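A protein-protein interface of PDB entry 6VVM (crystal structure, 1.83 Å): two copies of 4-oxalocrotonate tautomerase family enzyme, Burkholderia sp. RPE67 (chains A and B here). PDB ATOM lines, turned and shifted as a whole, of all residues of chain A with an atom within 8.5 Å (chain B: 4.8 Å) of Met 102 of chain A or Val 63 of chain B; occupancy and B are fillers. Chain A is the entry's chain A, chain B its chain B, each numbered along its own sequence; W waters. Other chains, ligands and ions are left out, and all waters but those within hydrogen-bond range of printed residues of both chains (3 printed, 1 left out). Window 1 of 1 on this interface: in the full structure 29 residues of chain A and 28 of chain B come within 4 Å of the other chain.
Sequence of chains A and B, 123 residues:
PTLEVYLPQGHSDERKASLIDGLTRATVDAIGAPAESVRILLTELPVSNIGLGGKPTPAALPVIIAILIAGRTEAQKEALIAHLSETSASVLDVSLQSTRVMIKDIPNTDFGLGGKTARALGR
The guanidinium group (NH1) of Arg 100 of chain B lies close to the guanidinium group (NH1) of Arg 100 of chain A, at 2.8 Å. NE of Arg 100 of chain A sits at hydrogen-bond distance from O of Ala 60 of chain B. The side-chain amide nitrogen of Asn 49 of chain B sits at hydrogen-bond distance from the backbone carbonyl oxygen of Ile 103 of chain A, at 2.9 Å. O of Ala 60 of chain A is in hydrogen-bond range of NE of Arg 100 of chain B (3.0 Å). OH of Tyr 6 of chain B sits at hydrogen-bond distance from NZ of Lys 104 of chain A. The side-chain carboxylate of Asp 105 of chain A lies within hydrogen-bond range of the side-chain amide nitrogen of Asn 49 of chain B (2.8 Å).
The backbone carbonyl oxygen of Ala 66 of chain A lies within hydrogen-bond range of the backbone NH of Lys 104 of chain A, 2.8 Å away. N of Glu 4 of chain B lies within hydrogen-bond range of O of Ile 65 of chain B. N of Tyr 6 of chain B is in hydrogen-bond range of O of Val 63 of chain B (3.0 Å).
CG of Tyr 6 of chain A touches CE of Met 102 of chain B (3.5 Å). Leu 61 of chain A touches Met 102 of chain B (CD2 to CG, 3.997 Å). Ile 65 of chain A touches Tyr 6 of chain B. Val 101 of chain A touches Asn 49 of chain B (O to O, 3.6 Å). Met 102 of chain A touches Tyr 6 of chain B. Met 102 of chain A touches Leu 61 of chain B (SD to CD2, 3.7 Å). Leu 45 of chain B touches Ile 103 of chain A.
Of the printed residues of chain B, Leu 61 of chain A touches Met 102. Of the printed residues of chain B, Val 63 of chain A touches Met 102 (3.9 Å). Met 102 of chain A touches five residues of chain B. Printed residues of chain A within 4 Å of Leu 45 of chain B: Met 102 (3.7 Å) and Ile 103 (3.5 Å). Val 63 of chain B touches just one residue of chain A: Met 102. The nearest printed residue of chain B that does not touch Ile 65 of chain A is Met 102 of chain B (5.7 Å).
Of the 25 printed residues of chain A, 12 touch a printed residue of chain B. Hydrophobic or aromatic side chains of chain A that line the printed part of chain B: Tyr 6, Ala 60, Leu 61, Val 63, Ile 65, Met 102 and Ile 103. Of the 13 printed residues of chain B, 9 touch a printed residue of chain A. Hydrophobic or aromatic side chains of chain B within 4 Å of the printed part of chain A: Tyr 6, Leu 45, Ala 60, Leu 61, Val 63, Ile 65 and Met 102. Among the printed residues, 20 pairs touch across the chains. Among the printed residues, no Asp or Glu carboxylate lies within 4 Å of a Lys or Arg side-chain nitrogen of the other chain.
Tyr 6 of chain A touches Ile 65 of chain B, and with the chains exchanged Ile 65 of chain A touches Tyr 6 of chain B. Ala 60 of chain A touches Arg 100 of chain B, and with the chains exchanged Arg 100 of chain A touches Ala 60 of chain B. Val 63 of chain A touches Met 102 of chain B, and with the chains exchanged Met 102 of chain A touches Val 63 of chain B. 10 positions are printed for both chains.
Water W1 lies within hydrogen-bond range of the side-chain amino group of Lys 104 of chain A (2.6 Å), the side-chain hydroxyl of Tyr 6 of chain B (2.7 Å) and the side-chain carboxylate of Glu 4 of chain B (3.1 Å). Water W3 lies within hydrogen-bond range of the guanidinium group of Arg 100 of chain A (2.6 Å) and the guanidinium group of Arg 100 of chain B (3.2 Å).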
ATOM      1  N   THR A   2      18.271  -5.556  -0.150  1.00  0.00           N
ATOM      2  CA  THR A   2      17.546  -6.008   1.025  1.00  0.00           C
ATOM      3  C   THR A   2      18.460  -5.831   2.230  1.00  0.00           C
ATOM      4  O   THR A   2      19.538  -6.428   2.284  1.00  0.00           O
ATOM      5  CB  THR A   2      17.111  -7.474   0.905  1.00  0.00           C
ATOM      6  OG1 THR A   2      16.235  -7.652  -0.218  1.00  0.00           O
ATOM      7  CG2 THR A   2      16.397  -7.901   2.175  1.00  0.00           C
ATOM      8  N   LEU A   3      18.041  -4.999   3.177  1.00  0.00           N
ATOM      9  CA  LEU A   3      18.795  -4.761   4.399  1.00  0.00           C
ATOM     10  C   LEU A   3      18.120  -5.467   5.566  1.00  0.00           C
ATOM     11  O   LEU A   3      16.891  -5.456   5.692  1.00  0.00           O
ATOM     12  CB  LEU A   3      18.912  -3.266   4.713  1.00  0.00           C
ATOM     13  CG  LEU A   3      19.275  -2.314   3.574  1.00  0.00           C
ATOM     14  CD1 LEU A   3      19.528  -0.929   4.147  1.00  0.00           C
ATOM     15  CD2 LEU A   3      20.507  -2.846   2.828  1.00  0.00           C
ATOM     16  N   GLU A   4      18.925  -6.062   6.439  1.00  0.00           N
ATOM     17  CA  GLU A   4      18.404  -6.636   7.671  1.00  0.00           C
ATOM     18  C   GLU A   4      19.222  -6.051   8.808  1.00  0.00           C
ATOM     19  O   GLU A   4      20.453  -6.150   8.802  1.00  0.00           O
ATOM     20  CB  GLU A   4      18.453  -8.176   7.671  1.00  0.00           C
ATOM     21  CG  GLU A   4      18.137  -8.749   9.065  1.00  0.00           C
ATOM     22  CD  GLU A   4      17.870 -10.246   9.124  1.00  0.00           C
ATOM     23  OE1 GLU A   4      18.320 -11.002   8.230  1.00  0.00           O
ATOM     24  OE2 GLU A   4      17.195 -10.662  10.096  1.00  0.00           O
ATOM     25  N   TYR A   6      19.882  -6.161  12.788  1.00  0.00           N
ATOM     26  CA  TYR A   6      19.760  -6.741  14.119  1.00  0.00           C
ATOM     27  C   TYR A   6      19.907  -5.634  15.160  1.00  0.00           C
ATOM     28  O   TYR A   6      20.941  -4.951  15.213  1.00  0.00           O
ATOM     29  CB  TYR A   6      20.813  -7.820  14.320  1.00  0.00           C
ATOM     30  CG  TYR A   6      20.484  -9.100  13.599  1.00  0.00           C
ATOM     31  CD1 TYR A   6      20.832  -9.280  12.266  1.00  0.00           C
ATOM     32  CD2 TYR A   6      19.811 -10.120  14.249  1.00  0.00           C
ATOM     33  CE1 TYR A   6      20.534 -10.448  11.608  1.00  0.00           C
ATOM     34  CE2 TYR A   6      19.511 -11.298  13.606  1.00  0.00           C
ATOM     35  CZ  TYR A   6      19.873 -11.462  12.290  1.00  0.00           C
ATOM     36  OH  TYR A   6      19.565 -12.646  11.667  1.00  0.00           O
ATOM     37  N   GLY A  51      24.801 -11.846  21.997  1.00  0.00           N
ATOM     38  CA  GLY A  51      26.086 -12.086  22.634  1.00  0.00           C
ATOM     39  C   GLY A  51      27.232 -11.222  22.143  1.00  0.00           C
ATOM     40  O   GLY A  51      27.429 -11.055  20.936  1.00  0.00           O
ATOM     41  N   ALA A  60      26.157  -5.678  21.613  1.00  0.00           N
ATOM     42  CA  ALA A  60      26.659  -6.379  20.438  1.00  0.00           C
ATOM     43  C   ALA A  60      26.123  -5.788  19.146  1.00  0.00           C
ATOM     44  O   ALA A  60      26.732  -5.986  18.088  1.00  0.00           O
ATOM     45  CB  ALA A  60      26.284  -7.858  20.496  1.00  0.00           C
ATOM     46  N   LEU A  61      24.999  -5.090  19.217  1.00  0.00           N
ATOM     47  CA  LEU A  61      24.262  -4.555  18.091  1.00  0.00           C
ATOM     48  C   LEU A  61      24.560  -3.071  17.945  1.00  0.00           C
ATOM     49  O   LEU A  61      25.014  -2.428  18.896  1.00  0.00           O
ATOM     50  CB  LEU A  61      22.764  -4.804  18.307  1.00  0.00           C
ATOM     51  CG  LEU A  61      22.492  -6.310  18.534  1.00  0.00           C
ATOM     52  CD1 LEU A  61      21.016  -6.642  18.542  1.00  0.00           C
ATOM     53  CD2 LEU A  61      23.208  -7.170  17.508  1.00  0.00           C
ATOM     54  N   PRO A  62      24.313  -2.482  16.764  1.00  0.00           N
ATOM     55  CA  PRO A  62      23.640  -3.103  15.609  1.00  0.00           C
ATOM     56  C   PRO A  62      24.530  -3.808  14.579  1.00  0.00           C
ATOM     57  O   PRO A  62      25.659  -3.404  14.331  1.00  0.00           O
ATOM     58  CB  PRO A  62      22.934  -1.917  14.953  1.00  0.00           C
ATOM     59  CG  PRO A  62      23.828  -0.748  15.239  1.00  0.00           C
ATOM     60  CD  PRO A  62      24.617  -1.058  16.520  1.00  0.00           C
ATOM     61  N   VAL A  63      23.986  -4.866  13.985  1.00  0.00           N
ATOM     62  CA  VAL A  63      24.610  -5.574  12.874  1.00  0.00           C
ATOM     63  C   VAL A  63      23.693  -5.418  11.668  1.00  0.00           C
ATOM     64  O   VAL A  63      22.501  -5.730  11.745  1.00  0.00           O
ATOM     65  CB  VAL A  63      24.843  -7.056  13.200  1.00  0.00           C
ATOM     66  CG1 VAL A  63      25.320  -7.812  11.950  1.00  0.00           C
ATOM     67  CG2 VAL A  63      25.845  -7.189  14.358  1.00  0.00           C
ATOM     68  N   ILE A  64      24.231  -4.902  10.572  1.00  0.00           N
ATOM     69  CA  ILE A  64      23.454  -4.687   9.356  1.00  0.00           C
ATOM     70  C   ILE A  64      23.960  -5.646   8.294  1.00  0.00           C
ATOM     71  O   ILE A  64      25.150  -5.637   7.959  1.00  0.00           O
ATOM     72  CB  ILE A  64      23.545  -3.235   8.862  1.00  0.00           C
ATOM     73  CG1 ILE A  64      23.152  -2.235   9.959  1.00  0.00           C
ATOM     74  CG2 ILE A  64      22.634  -3.061   7.664  1.00  0.00           C
ATOM     75  CD1 ILE A  64      24.348  -1.630  10.745  1.00  0.00           C
ATOM     76  N   ILE A  65      23.059  -6.466   7.756  1.00  0.00           N
ATOM     77  CA  ILE A  65      23.353  -7.289   6.595  1.00  0.00           C
ATOM     78  C   ILE A  65      22.703  -6.638   5.387  1.00  0.00           C
ATOM     79  O   ILE A  65      21.499  -6.344   5.406  1.00  0.00           O
ATOM     80  CB  ILE A  65      22.852  -8.728   6.788  1.00  0.00           C
ATOM     81  CG1 ILE A  65      23.514  -9.351   8.019  1.00  0.00           C
ATOM     82  CG2 ILE A  65      23.094  -9.562   5.537  1.00  0.00           C
ATOM     83  CD1 ILE A  65      22.843 -10.631   8.495  1.00  0.00           C
ATOM     84  N   ALA A  66      23.499  -6.393   4.353  1.00  0.00           N
ATOM     85  CA  ALA A  66      23.039  -5.754   3.124  1.00  0.00           C
ATOM     86  C   ALA A  66      23.260  -6.718   1.974  1.00  0.00           C
ATOM     87  O   ALA A  66      24.400  -7.106   1.700  1.00  0.00           O
ATOM     88  CB  ALA A  66      23.781  -4.441   2.865  1.00  0.00           C
ATOM     89  N   ILE A  67      22.175  -7.090   1.303  1.00  0.00           N
ATOM     90  CA  ILE A  67      22.208  -8.036   0.200  1.00  0.00           C
ATOM     91  C   ILE A  67      22.016  -7.280  -1.106  1.00  0.00           C
ATOM     92  O   ILE A  67      20.974  -6.646  -1.317  1.00  0.00           O
ATOM     93  CB  ILE A  67      21.141  -9.121   0.370  1.00  0.00           C
ATOM     94  CG1 ILE A  67      21.367  -9.824   1.715  1.00  0.00           C
ATOM     95  CG2 ILE A  67      21.195 -10.087  -0.805  1.00  0.00           C
ATOM     96  CD1 ILE A  67      20.457 -11.004   1.976  1.00  0.00           C
ATOM     97  N   LEU A  68      23.014  -7.372  -1.985  1.00  0.00           N
ATOM     98  CA  LEU A  68      23.071  -6.628  -3.243  1.00  0.00           C
ATOM     99  C   LEU A  68      23.254  -7.583  -4.408  1.00  0.00           C
ATOM    100  O   LEU A  68      23.916  -8.613  -4.270  1.00  0.00           O
ATOM    101  CB  LEU A  68      24.246  -5.649  -3.254  1.00  0.00           C
ATOM    102  CG  LEU A  68      24.450  -4.726  -2.055  1.00  0.00           C
ATOM    103  CD1 LEU A  68      25.763  -3.971  -2.207  1.00  0.00           C
ATOM    104  CD2 LEU A  68      23.290  -3.762  -1.968  1.00  0.00           C
ATOM    105  N   LEU A  80      28.716   2.483   1.095  1.00  0.00           N
ATOM    106  CA  LEU A  80      27.581   1.826   1.728  1.00  0.00           C
ATOM    107  C   LEU A  80      27.872   1.512   3.194  1.00  0.00           C
ATOM    108  O   LEU A  80      27.060   1.827   4.071  1.00  0.00           O
ATOM    109  CB  LEU A  80      27.204   0.560   0.957  1.00  0.00           C
ATOM    110  CG  LEU A  80      25.908  -0.115   1.422  1.00  0.00           C
ATOM    111  CD1 LEU A  80      24.694   0.823   1.352  1.00  0.00           C
ATOM    112  CD2 LEU A  80      25.656  -1.381   0.634  1.00  0.00           C
ATOM    113  N   ILE A  81      29.041   0.917   3.478  1.00  0.00           N
ATOM    114  CA  ILE A  81      29.433   0.637   4.866  1.00  0.00           C
ATOM    115  C   ILE A  81      29.437   1.919   5.696  1.00  0.00           C
ATOM    116  O   ILE A  81      28.919   1.956   6.817  1.00  0.00           O
ATOM    117  CB  ILE A  81      30.809  -0.056   4.909  1.00  0.00           C
ATOM    118  CG1 ILE A  81      30.685  -1.527   4.491  1.00  0.00           C
ATOM    119  CG2 ILE A  81      31.437   0.065   6.300  1.00  0.00           C
ATOM    120  CD1 ILE A  81      32.034  -2.190   4.203  1.00  0.00           C
ATOM    121  N   LEU A  84      25.595   3.350   6.022  1.00  0.00           N
ATOM    122  CA  LEU A  84      24.721   2.538   6.862  1.00  0.00           C
ATOM    123  C   LEU A  84      25.158   2.623   8.315  1.00  0.00           C
ATOM    124  O   LEU A  84      24.319   2.745   9.219  1.00  0.00           O
ATOM    125  CB  LEU A  84      24.707   1.081   6.379  1.00  0.00           C
ATOM    126  CG  LEU A  84      24.105   0.768   4.988  1.00  0.00           C
ATOM    127  CD1 LEU A  84      24.224  -0.745   4.667  1.00  0.00           C
ATOM    128  CD2 LEU A  84      22.654   1.214   4.903  1.00  0.00           C
ATOM    129  N   SER A  85      26.475   2.615   8.547  1.00  0.00           N
ATOM    130  CA  SER A  85      27.020   2.635   9.902  1.00  0.00           C
ATOM    131  C   SER A  85      26.689   3.957  10.588  1.00  0.00           C
ATOM    132  O   SER A  85      26.129   3.967  11.688  1.00  0.00           O
ATOM    133  CB  SER A  85      28.536   2.425   9.869  1.00  0.00           C
ATOM    134  OG  SER A  85      28.886   1.158   9.337  1.00  0.00           O
ATOM    135  N   THR A  99      28.979  -0.430  15.445  1.00  0.00           N
ATOM    136  CA  THR A  99      28.220  -0.896  14.289  1.00  0.00           C
ATOM    137  C   THR A  99      29.026  -1.877  13.438  1.00  0.00           C
ATOM    138  O   THR A  99      30.241  -1.731  13.262  1.00  0.00           O
ATOM    139  CB  THR A  99      27.763   0.278  13.414  1.00  0.00           C
ATOM    140  OG1 THR A  99      28.907   0.956  12.898  1.00  0.00           O
ATOM    141  CG2 THR A  99      26.895   1.284  14.212  1.00  0.00           C
ATOM    142  N   ARG A 100      28.325  -2.880  12.910  1.00  0.00           N
ATOM    143  CA  ARG A 100      28.875  -3.888  12.014  1.00  0.00           C
ATOM    144  C   ARG A 100      28.052  -3.921  10.740  1.00  0.00           C
ATOM    145  O   ARG A 100      26.822  -3.877  10.802  1.00  0.00           O
ATOM    146  CB  ARG A 100      28.841  -5.292  12.651  1.00  0.00           C
ATOM    147  CG  ARG A 100      29.653  -5.461  13.914  1.00  0.00           C
ATOM    148  CD  ARG A 100      31.094  -5.150  13.647  1.00  0.00           C
ATOM    149  NE  ARG A 100      32.016  -5.778  14.601  1.00  0.00           N
ATOM    150  CZ  ARG A 100      32.113  -5.441  15.885  1.00  0.00           C
ATOM    151  NH1 ARG A 100      33.011  -6.032  16.661  1.00  0.00           N
ATOM    152  NH2 ARG A 100      31.313  -4.519  16.400  1.00  0.00           N
ATOM    153  N   VAL A 101      28.723  -4.024   9.591  1.00  0.00           N
ATOM    154  CA  VAL A 101      28.049  -4.178   8.305  1.00  0.00           C
ATOM    155  C   VAL A 101      28.630  -5.381   7.578  1.00  0.00           C
ATOM    156  O   VAL A 101      29.852  -5.545   7.511  1.00  0.00           O
ATOM    157  CB  VAL A 101      28.183  -2.918   7.420  1.00  0.00           C
ATOM    158  CG1 VAL A 101      27.550  -3.175   6.033  1.00  0.00           C
ATOM    159  CG2 VAL A 101      27.545  -1.715   8.112  1.00  0.00           C
ATOM    160  N   MET A 102      27.753  -6.204   7.008  1.00  0.00           N
ATOM    161  CA  MET A 102      28.176  -7.336   6.197  1.00  0.00           C
ATOM    162  C   MET A 102      27.403  -7.327   4.888  1.00  0.00           C
ATOM    163  O   MET A 102      26.166  -7.293   4.888  1.00  0.00           O
ATOM    164  CB  MET A 102      27.962  -8.659   6.951  1.00  0.00           C
ATOM    165  CG  MET A 102      28.975  -8.890   8.042  1.00  0.00           C
ATOM    166  SD  MET A 102      28.263  -9.592   9.541  1.00  0.00           S
ATOM    167  CE  MET A 102      27.212 -10.921   8.956  1.00  0.00           C
ATOM    168  N   ILE A 103      28.127  -7.321   3.774  1.00  0.00           N
ATOM    169  CA  ILE A 103      27.530  -7.197   2.448  1.00  0.00           C
ATOM    170  C   ILE A 103      27.599  -8.540   1.748  1.00  0.00           C
ATOM    171  O   ILE A 103      28.687  -9.104   1.587  1.00  0.00           O
ATOM    172  CB  ILE A 103      28.233  -6.122   1.600  1.00  0.00           C
ATOM    173  CG1 ILE A 103      28.107  -4.744   2.266  1.00  0.00           C
ATOM    174  CG2 ILE A 103      27.649  -6.112   0.182  1.00  0.00           C
ATOM    175  CD1 ILE A 103      28.881  -3.668   1.566  1.00  0.00           C
ATOM    176  N   LYS A 104      26.446  -9.033   1.306  1.00  0.00           N
ATOM    177  CA  LYS A 104      26.356 -10.238   0.493  1.00  0.00           C
ATOM    178  C   LYS A 104      26.126  -9.840  -0.960  1.00  0.00           C
ATOM    179  O   LYS A 104      25.159  -9.132  -1.266  1.00  0.00           O
ATOM    180  CB  LYS A 104      25.232 -11.151   0.974  1.00  0.00           C
ATOM    181  CG  LYS A 104      25.547 -11.913   2.255  1.00  0.00           C
ATOM    182  CD  LYS A 104      24.304 -12.564   2.831  1.00  0.00           C
ATOM    183  CE  LYS A 104      24.187 -14.023   2.424  1.00  0.00           C
ATOM    184  NZ  LYS A 104      24.029 -14.897   3.632  1.00  0.00           N
ATOM    185  N   ASP A 105      27.020 -10.281  -1.841  1.00  0.00           N
ATOM    186  CA  ASP A 105      26.864 -10.126  -3.280  1.00  0.00           C
ATOM    187  C   ASP A 105      26.148 -11.348  -3.843  1.00  0.00           C
ATOM    188  O   ASP A 105      26.542 -12.480  -3.549  1.00  0.00           O
ATOM    189  CB  ASP A 105      28.227  -9.976  -3.948  1.00  0.00           C
ATOM    190  CG  ASP A 105      28.917  -8.687  -3.565  1.00  0.00           C
ATOM    191  OD1 ASP A 105      28.296  -7.628  -3.741  1.00  0.00           O
ATOM    192  OD2 ASP A 105      30.066  -8.738  -3.080  1.00  0.00           O
ATOM    193  N   GLU B   4      24.456 -19.621  10.995  1.00  0.00           N
ATOM    194  CA  GLU B   4      25.130 -18.924   9.911  1.00  0.00           C
ATOM    195  C   GLU B   4      26.335 -18.199  10.488  1.00  0.00           C
ATOM    196  O   GLU B   4      26.176 -17.328  11.344  1.00  0.00           O
ATOM    197  CB  GLU B   4      24.209 -17.917   9.230  1.00  0.00           C
ATOM    198  CG  GLU B   4      22.796 -18.377   8.948  1.00  0.00           C
ATOM    199  CD  GLU B   4      21.929 -17.213   8.497  1.00  0.00           C
ATOM    200  OE1 GLU B   4      20.990 -16.833   9.234  1.00  0.00           O
ATOM    201  OE2 GLU B   4      22.220 -16.648   7.418  1.00  0.00           O
ATOM    202  N   VAL B   5      27.528 -18.533  10.004  1.00  0.00           N
ATOM    203  CA  VAL B   5      28.773 -18.026  10.564  1.00  0.00           C
ATOM    204  C   VAL B   5      29.467 -17.174   9.508  1.00  0.00           C
ATOM    205  O   VAL B   5      29.947 -17.698   8.494  1.00  0.00           O
ATOM    206  CB  VAL B   5      29.686 -19.163  11.040  1.00  0.00           C
ATOM    207  CG1 VAL B   5      30.935 -18.588  11.633  1.00  0.00           C
ATOM    208  CG2 VAL B   5      28.958 -20.047  12.043  1.00  0.00           C
ATOM    209  N   TYR B   6      29.559 -15.869   9.773  1.00  0.00           N
ATOM    210  CA  TYR B   6      30.215 -14.901   8.893  1.00  0.00           C
ATOM    211  C   TYR B   6      31.691 -14.777   9.255  1.00  0.00           C
ATOM    212  O   TYR B   6      32.032 -14.370  10.377  1.00  0.00           O
ATOM    213  CB  TYR B   6      29.530 -13.539   8.987  1.00  0.00           C
ATOM    214  CG  TYR B   6      28.182 -13.528   8.332  1.00  0.00           C
ATOM    215  CD1 TYR B   6      27.054 -13.961   9.021  1.00  0.00           C
ATOM    216  CD2 TYR B   6      28.033 -13.116   7.004  1.00  0.00           C
ATOM    217  CE1 TYR B   6      25.801 -13.961   8.413  1.00  0.00           C
ATOM    218  CE2 TYR B   6      26.784 -13.109   6.393  1.00  0.00           C
ATOM    219  CZ  TYR B   6      25.679 -13.528   7.099  1.00  0.00           C
ATOM    220  OH  TYR B   6      24.446 -13.532   6.477  1.00  0.00           O
ATOM    221  N   LEU B  45      33.268 -13.634   3.539  1.00  0.00           N
ATOM    222  CA  LEU B  45      33.080 -12.348   2.897  1.00  0.00           C
ATOM    223  C   LEU B  45      34.421 -11.700   2.587  1.00  0.00           C
ATOM    224  O   LEU B  45      35.354 -11.806   3.387  1.00  0.00           O
ATOM    225  CB  LEU B  45      32.264 -11.409   3.790  1.00  0.00           C
ATOM    226  CG  LEU B  45      30.827 -11.857   4.061  1.00  0.00           C
ATOM    227  CD1 LEU B  45      30.107 -10.823   4.891  1.00  0.00           C
ATOM    228  CD2 LEU B  45      30.078 -12.122   2.759  1.00  0.00           C
ATOM    229  N   ASN B  49      33.629  -6.143   1.828  1.00  0.00           N
ATOM    230  CA  ASN B  49      32.226  -6.319   2.179  1.00  0.00           C
ATOM    231  C   ASN B  49      31.972  -6.248   3.679  1.00  0.00           C
ATOM    232  O   ASN B  49      30.824  -6.381   4.103  1.00  0.00           O
ATOM    233  CB  ASN B  49      31.715  -7.675   1.649  1.00  0.00           C
ATOM    234  CG  ASN B  49      31.597  -7.727   0.119  1.00  0.00           C
ATOM    235  OD1 ASN B  49      32.316  -7.034  -0.606  1.00  0.00           O
ATOM    236  ND2 ASN B  49      30.697  -8.582  -0.375  1.00  0.00           N
ATOM    237  N   ALA B  60      35.637  -6.957  12.010  1.00  0.00           N
ATOM    238  CA  ALA B  60      34.220  -6.922  12.348  1.00  0.00           C
ATOM    239  C   ALA B  60      33.670  -8.305  12.673  1.00  0.00           C
ATOM    240  O   ALA B  60      32.609  -8.410  13.296  1.00  0.00           O
ATOM    241  CB  ALA B  60      33.419  -6.335  11.191  1.00  0.00           C
ATOM    242  N   LEU B  61      34.344  -9.353  12.235  1.00  0.00           N
ATOM    243  CA  LEU B  61      33.891 -10.728  12.338  1.00  0.00           C
ATOM    244  C   LEU B  61      34.691 -11.471  13.412  1.00  0.00           C
ATOM    245  O   LEU B  61      35.728 -10.985  13.875  1.00  0.00           O
ATOM    246  CB  LEU B  61      34.020 -11.402  10.964  1.00  0.00           C
ATOM    247  CG  LEU B  61      33.317 -10.639   9.821  1.00  0.00           C
ATOM    248  CD1 LEU B  61      33.459 -11.359   8.477  1.00  0.00           C
ATOM    249  CD2 LEU B  61      31.835 -10.374  10.122  1.00  0.00           C
ATOM    250  N   PRO B  62      34.223 -12.658  13.858  1.00  0.00           N
ATOM    251  CA  PRO B  62      33.077 -13.451  13.422  1.00  0.00           C
ATOM    252  C   PRO B  62      31.760 -13.020  14.048  1.00  0.00           C
ATOM    253  O   PRO B  62      31.717 -12.534  15.176  1.00  0.00           O
ATOM    254  CB  PRO B  62      33.450 -14.867  13.870  1.00  0.00           C
ATOM    255  CG  PRO B  62      34.206 -14.634  15.150  1.00  0.00           C
ATOM    256  CD  PRO B  62      34.949 -13.314  14.960  1.00  0.00           C
ATOM    257  N   VAL B  63      30.692 -13.181  13.275  1.00  0.00           N
ATOM    258  CA  VAL B  63      29.319 -13.001  13.732  1.00  0.00           C
ATOM    259  C   VAL B  63      28.584 -14.307  13.473  1.00  0.00           C
ATOM    260  O   VAL B  63      28.549 -14.785  12.330  1.00  0.00           O
ATOM    261  CB  VAL B  63      28.615 -11.852  13.001  1.00  0.00           C
ATOM    262  CG1 VAL B  63      27.151 -11.754  13.452  1.00  0.00           C
ATOM    263  CG2 VAL B  63      29.359 -10.537  13.220  1.00  0.00           C
ATOM    264  N   ILE B  64      27.983 -14.872  14.514  1.00  0.00           N
ATOM    265  CA  ILE B  64      27.238 -16.122  14.399  1.00  0.00           C
ATOM    266  C   ILE B  64      25.762 -15.826  14.609  1.00  0.00           C
ATOM    267  O   ILE B  64      25.381 -15.218  15.614  1.00  0.00           O
ATOM    268  CB  ILE B  64      27.730 -17.167  15.403  1.00  0.00           C
ATOM    269  CG1 ILE B  64      29.212 -17.447  15.161  1.00  0.00           C
ATOM    270  CG2 ILE B  64      26.893 -18.429  15.277  1.00  0.00           C
ATOM    271  CD1 ILE B  64      29.782 -18.513  16.084  1.00  0.00           C
ATOM    272  N   ILE B  65      24.940 -16.221  13.644  1.00  0.00           N
ATOM    273  CA  ILE B  65      23.488 -16.196  13.774  1.00  0.00           C
ATOM    274  C   ILE B  65      23.004 -17.623  14.018  1.00  0.00           C
ATOM    275  O   ILE B  65      23.189 -18.508  13.172  1.00  0.00           O
ATOM    276  CB  ILE B  65      22.833 -15.586  12.526  1.00  0.00           C
ATOM    277  CG1 ILE B  65      23.242 -14.109  12.405  1.00  0.00           C
ATOM    278  CG2 ILE B  65      21.324 -15.681  12.628  1.00  0.00           C
ATOM    279  CD1 ILE B  65      22.846 -13.462  11.102  1.00  0.00           C
ATOM    280  N   ARG B 100      30.629 -12.167  18.091  1.00  0.00           N
ATOM    281  CA  ARG B 100      29.240 -11.779  18.270  1.00  0.00           C
ATOM    282  C   ARG B 100      28.331 -12.959  17.955  1.00  0.00           C
ATOM    283  O   ARG B 100      28.557 -13.693  16.989  1.00  0.00           O
ATOM    284  CB  ARG B 100      28.880 -10.575  17.382  1.00  0.00           C
ATOM    285  CG  ARG B 100      29.100  -9.246  18.093  1.00  0.00           C
ATOM    286  CD  ARG B 100      29.267  -8.055  17.157  1.00  0.00           C
ATOM    287  NE  ARG B 100      29.572  -6.849  17.930  1.00  0.00           N
ATOM    288  CZ  ARG B 100      30.702  -6.655  18.611  1.00  0.00           C
ATOM    289  NH1 ARG B 100      31.651  -7.585  18.616  1.00  0.00           N
ATOM    290  NH2 ARG B 100      30.894  -5.531  19.293  1.00  0.00           N
ATOM    291  N   MET B 102      24.064 -13.863  17.671  1.00  0.00           N
ATOM    292  CA  MET B 102      22.665 -13.452  17.691  1.00  0.00           C
ATOM    293  C   MET B 102      21.805 -14.694  17.551  1.00  0.00           C
ATOM    294  O   MET B 102      21.997 -15.482  16.621  1.00  0.00           O
ATOM    295  CB  MET B 102      22.334 -12.466  16.571  1.00  0.00           C
ATOM    296  CG  MET B 102      22.934 -11.089  16.773  1.00  0.00           C
ATOM    297  SD  MET B 102      24.367 -10.893  15.710  1.00  0.00           S
ATOM    298  CE  MET B 102      23.579 -10.642  14.118  1.00  0.00           C
HETATM  299  O   HOH W   1      24.855 -16.065   5.806  1.00  0.00           O
HETATM  300  O   HOH W   2      28.841  -3.808  19.076  1.00  0.00           O
HETATM  301  O   HOH W   3      32.403  -2.925  18.208  1.00  0.00           O
